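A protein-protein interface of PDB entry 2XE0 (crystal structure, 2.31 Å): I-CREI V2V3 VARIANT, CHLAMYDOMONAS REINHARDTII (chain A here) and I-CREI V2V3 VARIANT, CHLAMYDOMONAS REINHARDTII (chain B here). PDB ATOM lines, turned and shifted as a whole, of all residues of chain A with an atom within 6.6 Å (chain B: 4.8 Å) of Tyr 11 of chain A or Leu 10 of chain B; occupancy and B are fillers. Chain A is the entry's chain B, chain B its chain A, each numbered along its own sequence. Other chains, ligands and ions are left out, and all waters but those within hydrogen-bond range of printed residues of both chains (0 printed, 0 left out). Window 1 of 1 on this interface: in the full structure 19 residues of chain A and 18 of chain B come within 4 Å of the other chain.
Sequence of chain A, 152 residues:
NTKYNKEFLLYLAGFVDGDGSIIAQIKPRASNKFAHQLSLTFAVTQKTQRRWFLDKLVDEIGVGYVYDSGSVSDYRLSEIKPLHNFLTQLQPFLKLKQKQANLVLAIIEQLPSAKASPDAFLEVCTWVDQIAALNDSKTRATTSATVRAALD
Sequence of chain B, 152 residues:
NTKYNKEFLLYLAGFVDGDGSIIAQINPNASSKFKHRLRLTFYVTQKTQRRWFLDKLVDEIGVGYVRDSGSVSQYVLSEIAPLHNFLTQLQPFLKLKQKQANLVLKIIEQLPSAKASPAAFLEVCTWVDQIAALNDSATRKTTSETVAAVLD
The backbone carbonyl oxygen (O) of Gly 14 of chain B lies close to the backbone NH (N) of Phe 15 of chain A (3.5 Å).
The side-chain amino group (NZ) of Lys 6 of chain A lies within salt-bridge range of the side-chain carboxylate (OE2) of Glu 7 of chain B, at 3.7 Å.
The side-chain hydroxyl (OH) of Tyr 11 of chain A sits at hydrogen-bond distance from the side-chain carboxylate (OD2) of Asp 17 of chain B, 2.5 Å away.
The side-chain carboxylate of Glu 7 of chain A lies within salt-bridge range of the side-chain amino group of Lys 6 of chain B, at 3.5 Å.
OD2 of Asp 17 of chain B sits at hydrogen-bond distance from N of Lys 95 of chain B, 2.9 Å away.
The side-chain carboxylate (OD1) of Asp 17 of chain B sits at hydrogen-bond distance from the backbone NH (N) of Leu 96 of chain B (3.3 Å).
Leu 10 of chain B touches Leu 10 of chain A (CB to CB, 3.9 Å).
CA of Tyr 11 of chain B touches O of Leu 10 of chain A, 3.5 Å away.
Tyr 11 of chain A touches Ala 13 of chain B (CE1 to C, 3.8 Å).
Tyr 11 of chain A touches Gly 14 of chain B.
O of Phe 93 of chain B touches CE1 of Tyr 11 of chain A, at 3.7 Å.
Tyr 11 of chain B touches Ala 13 of chain A.
Tyr 11 of chain B touches Gly 14 of chain A (CE1 to CA, 3.3 Å).
Gly 14 of chain A touches Gly 14 of chain B (C to C, 3.5 Å).
Phe 15 of chain A touches Asp 17 of chain B.
Phe 53 of chain A touches Leu 96 of chain B.
Tyr 11 of chain A touches six residues of chain B.
Of chain A, only Glu 7 (3.8 Å), Leu 10 (3.9 Å) and Tyr 11 (3.4 Å) come within 4 Å of Leu 10 of chain B.
Printed residues of chain A within 4 Å of Lys 95 of chain B: Tyr 11.
Of the printed residues of chain B, Phe 15 of chain A touches Gly 14, Asp 17 and Leu 96.
Of the printed residues of chain A, Tyr 11 of chain B touches Leu 10 (3.5 Å), Ala 13 (3.9 Å) and Gly 14 (3.3 Å).
Leu 9 of chain A touches none of the printed residues of chain B.
Leu 12 of chain A touches none of the printed residues of chain B.
The nearest residue of chain B that does not touch Tyr 11 of chain A is Tyr 11 of chain B (4.6 Å).
The nearest printed residue of chain B that does not touch Ala 13 of chain A is Gly 14 of chain B (6.1 Å).
Of the 13 printed residues of chain B, 10 touch a printed residue of chain A.
Printed residues of chain B that touch a printed residue of chain A: Lys 6, Glu 7, Leu 10, Tyr 11, Ala 13, Gly 14, Asp 17, Phe 93, Lys 95 and Leu 96.
Hydrophobic or aromatic side chains of chain B that line the printed part of chain A: Leu 10, Tyr 11 and Leu 96.
Along chain B the printed residues that touch a printed residue of chain A span positions 6 to 96.
Of the 12 printed residues of chain A, 8 touch a printed residue of chain B.
Printed residues of chain A that touch a printed residue of chain B: Lys 6, Glu 7, Leu 10, Tyr 11, Ala 13, Gly 14, Phe 15 and Phe 53.
Among the printed residues, Asp or Glu carboxylates within 4 Å of a Lys or Arg side-chain nitrogen of the other chain: Lys 6 of chain A with Glu 7 of chain B and Glu 7 of chain A with Lys 6 of chain B.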
ATOM      1  N   LYS A   6       8.454 -29.970   1.333  1.00  0.00           N
ATOM      2  CA  LYS A   6       8.051 -29.578   2.670  1.00  0.00           C
ATOM      3  C   LYS A   6       7.355 -28.238   2.775  1.00  0.00           C
ATOM      4  O   LYS A   6       6.475 -28.083   3.547  1.00  0.00           O
ATOM      5  CB  LYS A   6       9.243 -29.604   3.607  1.00  0.00           C
ATOM      6  CG  LYS A   6       8.902 -29.375   5.039  1.00  0.00           C
ATOM      7  CD  LYS A   6      10.065 -29.633   5.943  1.00  0.00           C
ATOM      8  CE  LYS A   6       9.895 -28.980   7.285  1.00  0.00           C
ATOM      9  NZ  LYS A   6      10.601 -29.667   8.382  1.00  0.00           N
ATOM     10  N   GLU A   7       7.782 -27.269   2.005  1.00  0.00           N
ATOM     11  CA  GLU A   7       7.136 -25.993   1.974  1.00  0.00           C
ATOM     12  C   GLU A   7       5.736 -26.111   1.444  1.00  0.00           C
ATOM     13  O   GLU A   7       4.862 -25.443   1.893  1.00  0.00           O
ATOM     14  CB  GLU A   7       7.945 -25.010   1.143  1.00  0.00           C
ATOM     15  CG  GLU A   7       9.000 -24.302   1.923  1.00  0.00           C
ATOM     16  CD  GLU A   7       9.400 -22.960   1.379  1.00  0.00           C
ATOM     17  OE1 GLU A   7       8.808 -22.456   0.430  1.00  0.00           O
ATOM     18  OE2 GLU A   7      10.344 -22.401   1.908  1.00  0.00           O
ATOM     19  N   PHE A   8       5.560 -26.925   0.428  1.00  0.00           N
ATOM     20  CA  PHE A   8       4.266 -27.187  -0.159  1.00  0.00           C
ATOM     21  C   PHE A   8       3.347 -27.881   0.828  1.00  0.00           C
ATOM     22  O   PHE A   8       2.220 -27.535   0.978  1.00  0.00           O
ATOM     23  CB  PHE A   8       4.453 -27.994  -1.444  1.00  0.00           C
ATOM     24  CG  PHE A   8       3.243 -28.741  -1.891  1.00  0.00           C
ATOM     25  CD1 PHE A   8       2.275 -28.128  -2.613  1.00  0.00           C
ATOM     26  CD2 PHE A   8       3.094 -30.063  -1.608  1.00  0.00           C
ATOM     27  CE1 PHE A   8       1.199 -28.793  -3.007  1.00  0.00           C
ATOM     28  CE2 PHE A   8       2.008 -30.712  -2.008  1.00  0.00           C
ATOM     29  CZ  PHE A   8       1.065 -30.076  -2.716  1.00  0.00           C
ATOM     30  N   LEU A   9       3.879 -28.850   1.524  1.00  0.00           N
ATOM     31  CA  LEU A   9       3.165 -29.568   2.537  1.00  0.00           C
ATOM     32  C   LEU A   9       2.738 -28.719   3.716  1.00  0.00           C
ATOM     33  O   LEU A   9       1.706 -28.936   4.272  1.00  0.00           O
ATOM     34  CB  LEU A   9       3.971 -30.758   3.015  1.00  0.00           C
ATOM     35  CG  LEU A   9       4.077 -31.961   2.107  1.00  0.00           C
ATOM     36  CD1 LEU A   9       4.975 -32.960   2.720  1.00  0.00           C
ATOM     37  CD2 LEU A   9       2.743 -32.543   1.834  1.00  0.00           C
ATOM     38  N   LEU A  10       3.572 -27.788   4.122  1.00  0.00           N
ATOM     39  CA  LEU A  10       3.201 -26.857   5.159  1.00  0.00           C
ATOM     40  C   LEU A  10       2.067 -25.947   4.762  1.00  0.00           C
ATOM     41  O   LEU A  10       1.141 -25.782   5.492  1.00  0.00           O
ATOM     42  CB  LEU A  10       4.398 -26.041   5.612  1.00  0.00           C
ATOM     43  CG  LEU A  10       5.200 -26.601   6.766  1.00  0.00           C
ATOM     44  CD1 LEU A  10       6.559 -26.097   6.744  1.00  0.00           C
ATOM     45  CD2 LEU A  10       4.577 -26.246   8.007  1.00  0.00           C
ATOM     46  N   TYR A  11       2.142 -25.381   3.584  1.00  0.00           N
ATOM     47  CA  TYR A  11       1.074 -24.563   3.122  1.00  0.00           C
ATOM     48  C   TYR A  11      -0.212 -25.342   2.980  1.00  0.00           C
ATOM     49  O   TYR A  11      -1.213 -24.889   3.427  1.00  0.00           O
ATOM     50  CB  TYR A  11       1.425 -23.922   1.796  1.00  0.00           C
ATOM     51  CG  TYR A  11       0.277 -23.175   1.217  1.00  0.00           C
ATOM     52  CD1 TYR A  11       0.081 -21.879   1.527  1.00  0.00           C
ATOM     53  CD2 TYR A  11      -0.629 -23.782   0.380  1.00  0.00           C
ATOM     54  CE1 TYR A  11      -0.935 -21.219   1.037  1.00  0.00           C
ATOM     55  CE2 TYR A  11      -1.655 -23.115  -0.109  1.00  0.00           C
ATOM     56  CZ  TYR A  11      -1.811 -21.826   0.226  1.00  0.00           C
ATOM     57  OH  TYR A  11      -2.841 -21.096  -0.234  1.00  0.00           O
ATOM     58  N   LEU A  12      -0.170 -26.513   2.370  1.00  0.00           N
ATOM     59  CA  LEU A  12      -1.341 -27.331   2.157  1.00  0.00           C
ATOM     60  C   LEU A  12      -2.010 -27.831   3.414  1.00  0.00           C
ATOM     61  O   LEU A  12      -3.189 -27.871   3.486  1.00  0.00           O
ATOM     62  CB  LEU A  12      -1.043 -28.465   1.200  1.00  0.00           C
ATOM     63  CG  LEU A  12      -2.175 -29.386   0.761  1.00  0.00           C
ATOM     64  CD1 LEU A  12      -3.314 -28.651   0.209  1.00  0.00           C
ATOM     65  CD2 LEU A  12      -1.747 -30.417  -0.173  1.00  0.00           C
ATOM     66  N   ALA A  13      -1.243 -28.183   4.414  1.00  0.00           N
ATOM     67  CA  ALA A  13      -1.807 -28.609   5.659  1.00  0.00           C
ATOM     68  C   ALA A  13      -2.620 -27.510   6.307  1.00  0.00           C
ATOM     69  O   ALA A  13      -3.669 -27.753   6.785  1.00  0.00           O
ATOM     70  CB  ALA A  13      -0.751 -29.066   6.562  1.00  0.00           C
ATOM     71  N   GLY A  14      -2.135 -26.286   6.289  1.00  0.00           N
ATOM     72  CA  GLY A  14      -2.895 -25.179   6.773  1.00  0.00           C
ATOM     73  C   GLY A  14      -4.156 -24.968   5.983  1.00  0.00           C
ATOM     74  O   GLY A  14      -5.159 -24.711   6.544  1.00  0.00           O
ATOM     75  N   PHE A  15      -4.084 -25.079   4.678  1.00  0.00           N
ATOM     76  CA  PHE A  15      -5.247 -24.971   3.833  1.00  0.00           C
ATOM     77  C   PHE A  15      -6.305 -26.059   4.011  1.00  0.00           C
ATOM     78  O   PHE A  15      -7.451 -25.790   3.994  1.00  0.00           O
ATOM     79  CB  PHE A  15      -4.840 -24.829   2.379  1.00  0.00           C
ATOM     80  CG  PHE A  15      -5.920 -24.327   1.526  1.00  0.00           C
ATOM     81  CD1 PHE A  15      -6.087 -22.995   1.334  1.00  0.00           C
ATOM     82  CD2 PHE A  15      -6.815 -25.181   0.956  1.00  0.00           C
ATOM     83  CE1 PHE A  15      -7.083 -22.548   0.586  1.00  0.00           C
ATOM     84  CE2 PHE A  15      -7.805 -24.721   0.223  1.00  0.00           C
ATOM     85  CZ  PHE A  15      -7.940 -23.406   0.038  1.00  0.00           C
ATOM     86  N   VAL A  16      -5.866 -27.283   4.161  1.00  0.00           N
ATOM     87  CA  VAL A  16      -6.697 -28.419   4.442  1.00  0.00           C
ATOM     88  C   VAL A  16      -7.386 -28.318   5.795  1.00  0.00           C
ATOM     89  O   VAL A  16      -8.524 -28.624   5.935  1.00  0.00           O
ATOM     90  CB  VAL A  16      -5.866 -29.682   4.314  1.00  0.00           C
ATOM     91  CG1 VAL A  16      -6.543 -30.839   4.854  1.00  0.00           C
ATOM     92  CG2 VAL A  16      -5.528 -29.893   2.925  1.00  0.00           C
ATOM     93  N   PHE A  53      -7.395 -23.176  -8.526  1.00  0.00           N
ATOM     94  CA  PHE A  53      -6.623 -23.543  -7.360  1.00  0.00           C
ATOM     95  C   PHE A  53      -6.604 -25.033  -7.098  1.00  0.00           C
ATOM     96  O   PHE A  53      -5.594 -25.597  -6.804  1.00  0.00           O
ATOM     97  CB  PHE A  53      -7.152 -22.738  -6.169  1.00  0.00           C
ATOM     98  CG  PHE A  53      -6.403 -22.943  -4.899  1.00  0.00           C
ATOM     99  CD1 PHE A  53      -5.348 -22.160  -4.573  1.00  0.00           C
ATOM    100  CD2 PHE A  53      -6.775 -23.912  -4.019  1.00  0.00           C
ATOM    101  CE1 PHE A  53      -4.686 -22.360  -3.419  1.00  0.00           C
ATOM    102  CE2 PHE A  53      -6.102 -24.101  -2.893  1.00  0.00           C
ATOM    103  CZ  PHE A  53      -5.064 -23.323  -2.589  1.00  0.00           C
ATOM    104  N   LYS B   6       9.393 -19.084   9.608  1.00  0.00           N
ATOM    105  CA  LYS B   6       8.935 -19.337   8.264  1.00  0.00           C
ATOM    106  C   LYS B   6       7.908 -20.418   8.145  1.00  0.00           C
ATOM    107  O   LYS B   6       6.988 -20.293   7.411  1.00  0.00           O
ATOM    108  CB  LYS B   6      10.110 -19.692   7.373  1.00  0.00           C
ATOM    109  CG  LYS B   6       9.750 -19.847   5.948  1.00  0.00           C
ATOM    110  CD  LYS B   6      10.946 -19.728   5.086  1.00  0.00           C
ATOM    111  CE  LYS B   6      10.645 -20.035   3.675  1.00  0.00           C
ATOM    112  NZ  LYS B   6      11.512 -19.277   2.814  1.00  0.00           N
ATOM    113  N   GLU B   7       8.116 -21.507   8.845  1.00  0.00           N
ATOM    114  CA  GLU B   7       7.211 -22.619   8.841  1.00  0.00           C
ATOM    115  C   GLU B   7       5.855 -22.276   9.422  1.00  0.00           C
ATOM    116  O   GLU B   7       4.864 -22.750   8.986  1.00  0.00           O
ATOM    117  CB  GLU B   7       7.865 -23.806   9.491  1.00  0.00           C
ATOM    118  CG  GLU B   7       9.179 -24.123   8.828  1.00  0.00           C
ATOM    119  CD  GLU B   7       9.756 -25.445   9.235  1.00  0.00           C
ATOM    120  OE1 GLU B   7       9.376 -25.967  10.291  1.00  0.00           O
ATOM    121  OE2 GLU B   7      10.596 -25.970   8.499  1.00  0.00           O
ATOM    122  N   PHE B   8       5.851 -21.427  10.420  1.00  0.00           N
ATOM    123  CA  PHE B   8       4.648 -20.883  10.972  1.00  0.00           C
ATOM    124  C   PHE B   8       3.884 -20.048   9.961  1.00  0.00           C
ATOM    125  O   PHE B   8       2.703 -20.170   9.850  1.00  0.00           O
ATOM    126  CB  PHE B   8       5.023 -20.055  12.196  1.00  0.00           C
ATOM    127  CG  PHE B   8       3.960 -19.149  12.678  1.00  0.00           C
ATOM    128  CD1 PHE B   8       2.966 -19.608  13.467  1.00  0.00           C
ATOM    129  CD2 PHE B   8       3.960 -17.833  12.355  1.00  0.00           C
ATOM    130  CE1 PHE B   8       2.004 -18.771  13.899  1.00  0.00           C
ATOM    131  CE2 PHE B   8       2.988 -17.017  12.795  1.00  0.00           C
ATOM    132  CZ  PHE B   8       2.025 -17.482  13.571  1.00  0.00           C
ATOM    133  N   LEU B   9       4.582 -19.199   9.238  1.00  0.00           N
ATOM    134  CA  LEU B   9       4.001 -18.370   8.225  1.00  0.00           C
ATOM    135  C   LEU B   9       3.431 -19.142   7.066  1.00  0.00           C
ATOM    136  O   LEU B   9       2.423 -18.780   6.552  1.00  0.00           O
ATOM    137  CB  LEU B   9       4.983 -17.322   7.746  1.00  0.00           C
ATOM    138  CG  LEU B   9       5.309 -16.146   8.648  1.00  0.00           C
ATOM    139  CD1 LEU B   9       6.477 -15.399   8.150  1.00  0.00           C
ATOM    140  CD2 LEU B   9       4.160 -15.259   8.851  1.00  0.00           C
ATOM    141  N   LEU B  10       4.120 -20.192   6.661  1.00  0.00           N
ATOM    142  CA  LEU B  10       3.670 -21.090   5.620  1.00  0.00           C
ATOM    143  C   LEU B  10       2.389 -21.831   5.961  1.00  0.00           C
ATOM    144  O   LEU B  10       1.491 -21.864   5.174  1.00  0.00           O
ATOM    145  CB  LEU B  10       4.751 -22.128   5.373  1.00  0.00           C
ATOM    146  CG  LEU B  10       5.603 -22.272   4.129  1.00  0.00           C
ATOM    147  CD1 LEU B  10       5.371 -21.320   3.059  1.00  0.00           C
ATOM    148  CD2 LEU B  10       7.008 -22.386   4.462  1.00  0.00           C
ATOM    149  N   TYR B  11       2.305 -22.415   7.137  1.00  0.00           N
ATOM    150  CA  TYR B  11       1.073 -23.012   7.566  1.00  0.00           C
ATOM    151  C   TYR B  11      -0.057 -22.017   7.712  1.00  0.00           C
ATOM    152  O   TYR B  11      -1.113 -22.269   7.268  1.00  0.00           O
ATOM    153  CB  TYR B  11       1.272 -23.770   8.866  1.00  0.00           C
ATOM    154  CG  TYR B  11       0.005 -24.270   9.467  1.00  0.00           C
ATOM    155  CD1 TYR B  11      -0.457 -25.513   9.191  1.00  0.00           C
ATOM    156  CD2 TYR B  11      -0.746 -23.485  10.298  1.00  0.00           C
ATOM    157  CE1 TYR B  11      -1.596 -25.957   9.720  1.00  0.00           C
ATOM    158  CE2 TYR B  11      -1.896 -23.934  10.824  1.00  0.00           C
ATOM    159  CZ  TYR B  11      -2.315 -25.175  10.529  1.00  0.00           C
ATOM    160  OH  TYR B  11      -3.456 -25.659  11.032  1.00  0.00           O
ATOM    161  N   LEU B  12       0.204 -20.882   8.326  1.00  0.00           N
ATOM    162  CA  LEU B  12      -0.783 -19.857   8.558  1.00  0.00           C
ATOM    163  C   LEU B  12      -1.320 -19.272   7.284  1.00  0.00           C
ATOM    164  O   LEU B  12      -2.465 -19.014   7.172  1.00  0.00           O
ATOM    165  CB  LEU B  12      -0.229 -18.773   9.466  1.00  0.00           C
ATOM    166  CG  LEU B  12      -1.209 -17.763  10.009  1.00  0.00           C
ATOM    167  CD1 LEU B  12      -2.345 -18.411  10.714  1.00  0.00           C
ATOM    168  CD2 LEU B  12      -0.538 -16.789  10.847  1.00  0.00           C
ATOM    169  N   ALA B  13      -0.452 -19.109   6.320  1.00  0.00           N
ATOM    170  CA  ALA B  13      -0.820 -18.610   5.041  1.00  0.00           C
ATOM    171  C   ALA B  13      -1.778 -19.547   4.377  1.00  0.00           C
ATOM    172  O   ALA B  13      -2.678 -19.122   3.749  1.00  0.00           O
ATOM    173  CB  ALA B  13       0.356 -18.416   4.213  1.00  0.00           C
ATOM    174  N   GLY B  14      -1.562 -20.833   4.510  1.00  0.00           N
ATOM    175  CA  GLY B  14      -2.520 -21.777   4.028  1.00  0.00           C
ATOM    176  C   GLY B  14      -3.840 -21.734   4.739  1.00  0.00           C
ATOM    177  O   GLY B  14      -4.837 -21.731   4.108  1.00  0.00           O
ATOM    178  N   ASP B  17      -5.708 -18.560   3.857  1.00  0.00           N
ATOM    179  CA  ASP B  17      -6.256 -18.652   2.542  1.00  0.00           C
ATOM    180  C   ASP B  17      -7.547 -19.414   2.629  1.00  0.00           C
ATOM    181  O   ASP B  17      -8.436 -19.159   1.881  1.00  0.00           O
ATOM    182  CB  ASP B  17      -5.286 -19.304   1.563  1.00  0.00           C
ATOM    183  CG  ASP B  17      -4.403 -18.316   0.842  1.00  0.00           C
ATOM    184  OD1 ASP B  17      -4.689 -17.160   0.781  1.00  0.00           O
ATOM    185  OD2 ASP B  17      -3.392 -18.722   0.324  1.00  0.00           O
ATOM    186  N   PHE B  93       3.767 -15.813   1.158  1.00  0.00           N
ATOM    187  CA  PHE B  93       3.224 -17.150   1.198  1.00  0.00           C
ATOM    188  C   PHE B  93       1.757 -17.330   0.827  1.00  0.00           C
ATOM    189  O   PHE B  93       1.345 -18.407   0.559  1.00  0.00           O
ATOM    190  CB  PHE B  93       3.572 -17.780   2.535  1.00  0.00           C
ATOM    191  CG  PHE B  93       5.014 -17.681   2.868  1.00  0.00           C
ATOM    192  CD1 PHE B  93       5.955 -18.218   2.045  1.00  0.00           C
ATOM    193  CD2 PHE B  93       5.437 -17.026   3.973  1.00  0.00           C
ATOM    194  CE1 PHE B  93       7.244 -18.121   2.327  1.00  0.00           C
ATOM    195  CE2 PHE B  93       6.752 -16.929   4.238  1.00  0.00           C
ATOM    196  CZ  PHE B  93       7.643 -17.482   3.417  1.00  0.00           C
ATOM    197  N   LYS B  95      -1.682 -17.264  -1.454  1.00  0.00           N
ATOM    198  CA  LYS B  95      -2.054 -17.426  -2.837  1.00  0.00           C
ATOM    199  C   LYS B  95      -3.385 -16.793  -3.173  1.00  0.00           C
ATOM    200  O   LYS B  95      -3.457 -15.909  -3.971  1.00  0.00           O
ATOM    201  CB  LYS B  95      -2.041 -18.893  -3.203  1.00  0.00           C
ATOM    202  CG  LYS B  95      -0.909 -19.598  -2.595  1.00  0.00           C
ATOM    203  CD  LYS B  95      -0.688 -20.930  -3.190  1.00  0.00           C
ATOM    204  CE  LYS B  95       0.756 -21.254  -3.153  1.00  0.00           C
ATOM    205  NZ  LYS B  95       1.080 -22.532  -2.509  1.00  0.00           N
ATOM    206  N   LEU B  96      -4.439 -17.238  -2.542  1.00  0.00           N
ATOM    207  CA  LEU B  96      -5.749 -16.682  -2.739  1.00  0.00           C
ATOM    208  C   LEU B  96      -5.869 -15.250  -2.305  1.00  0.00           C
ATOM    209  O   LEU B  96      -6.608 -14.503  -2.868  1.00  0.00           O
ATOM    210  CB  LEU B  96      -6.786 -17.540  -2.047  1.00  0.00           C
ATOM    211  CG  LEU B  96      -6.785 -19.010  -2.415  1.00  0.00           C
ATOM    212  CD1 LEU B  96      -7.947 -19.700  -1.839  1.00  0.00           C
ATOM    213  CD2 LEU B  96      -6.780 -19.188  -3.865  1.00  0.00           C
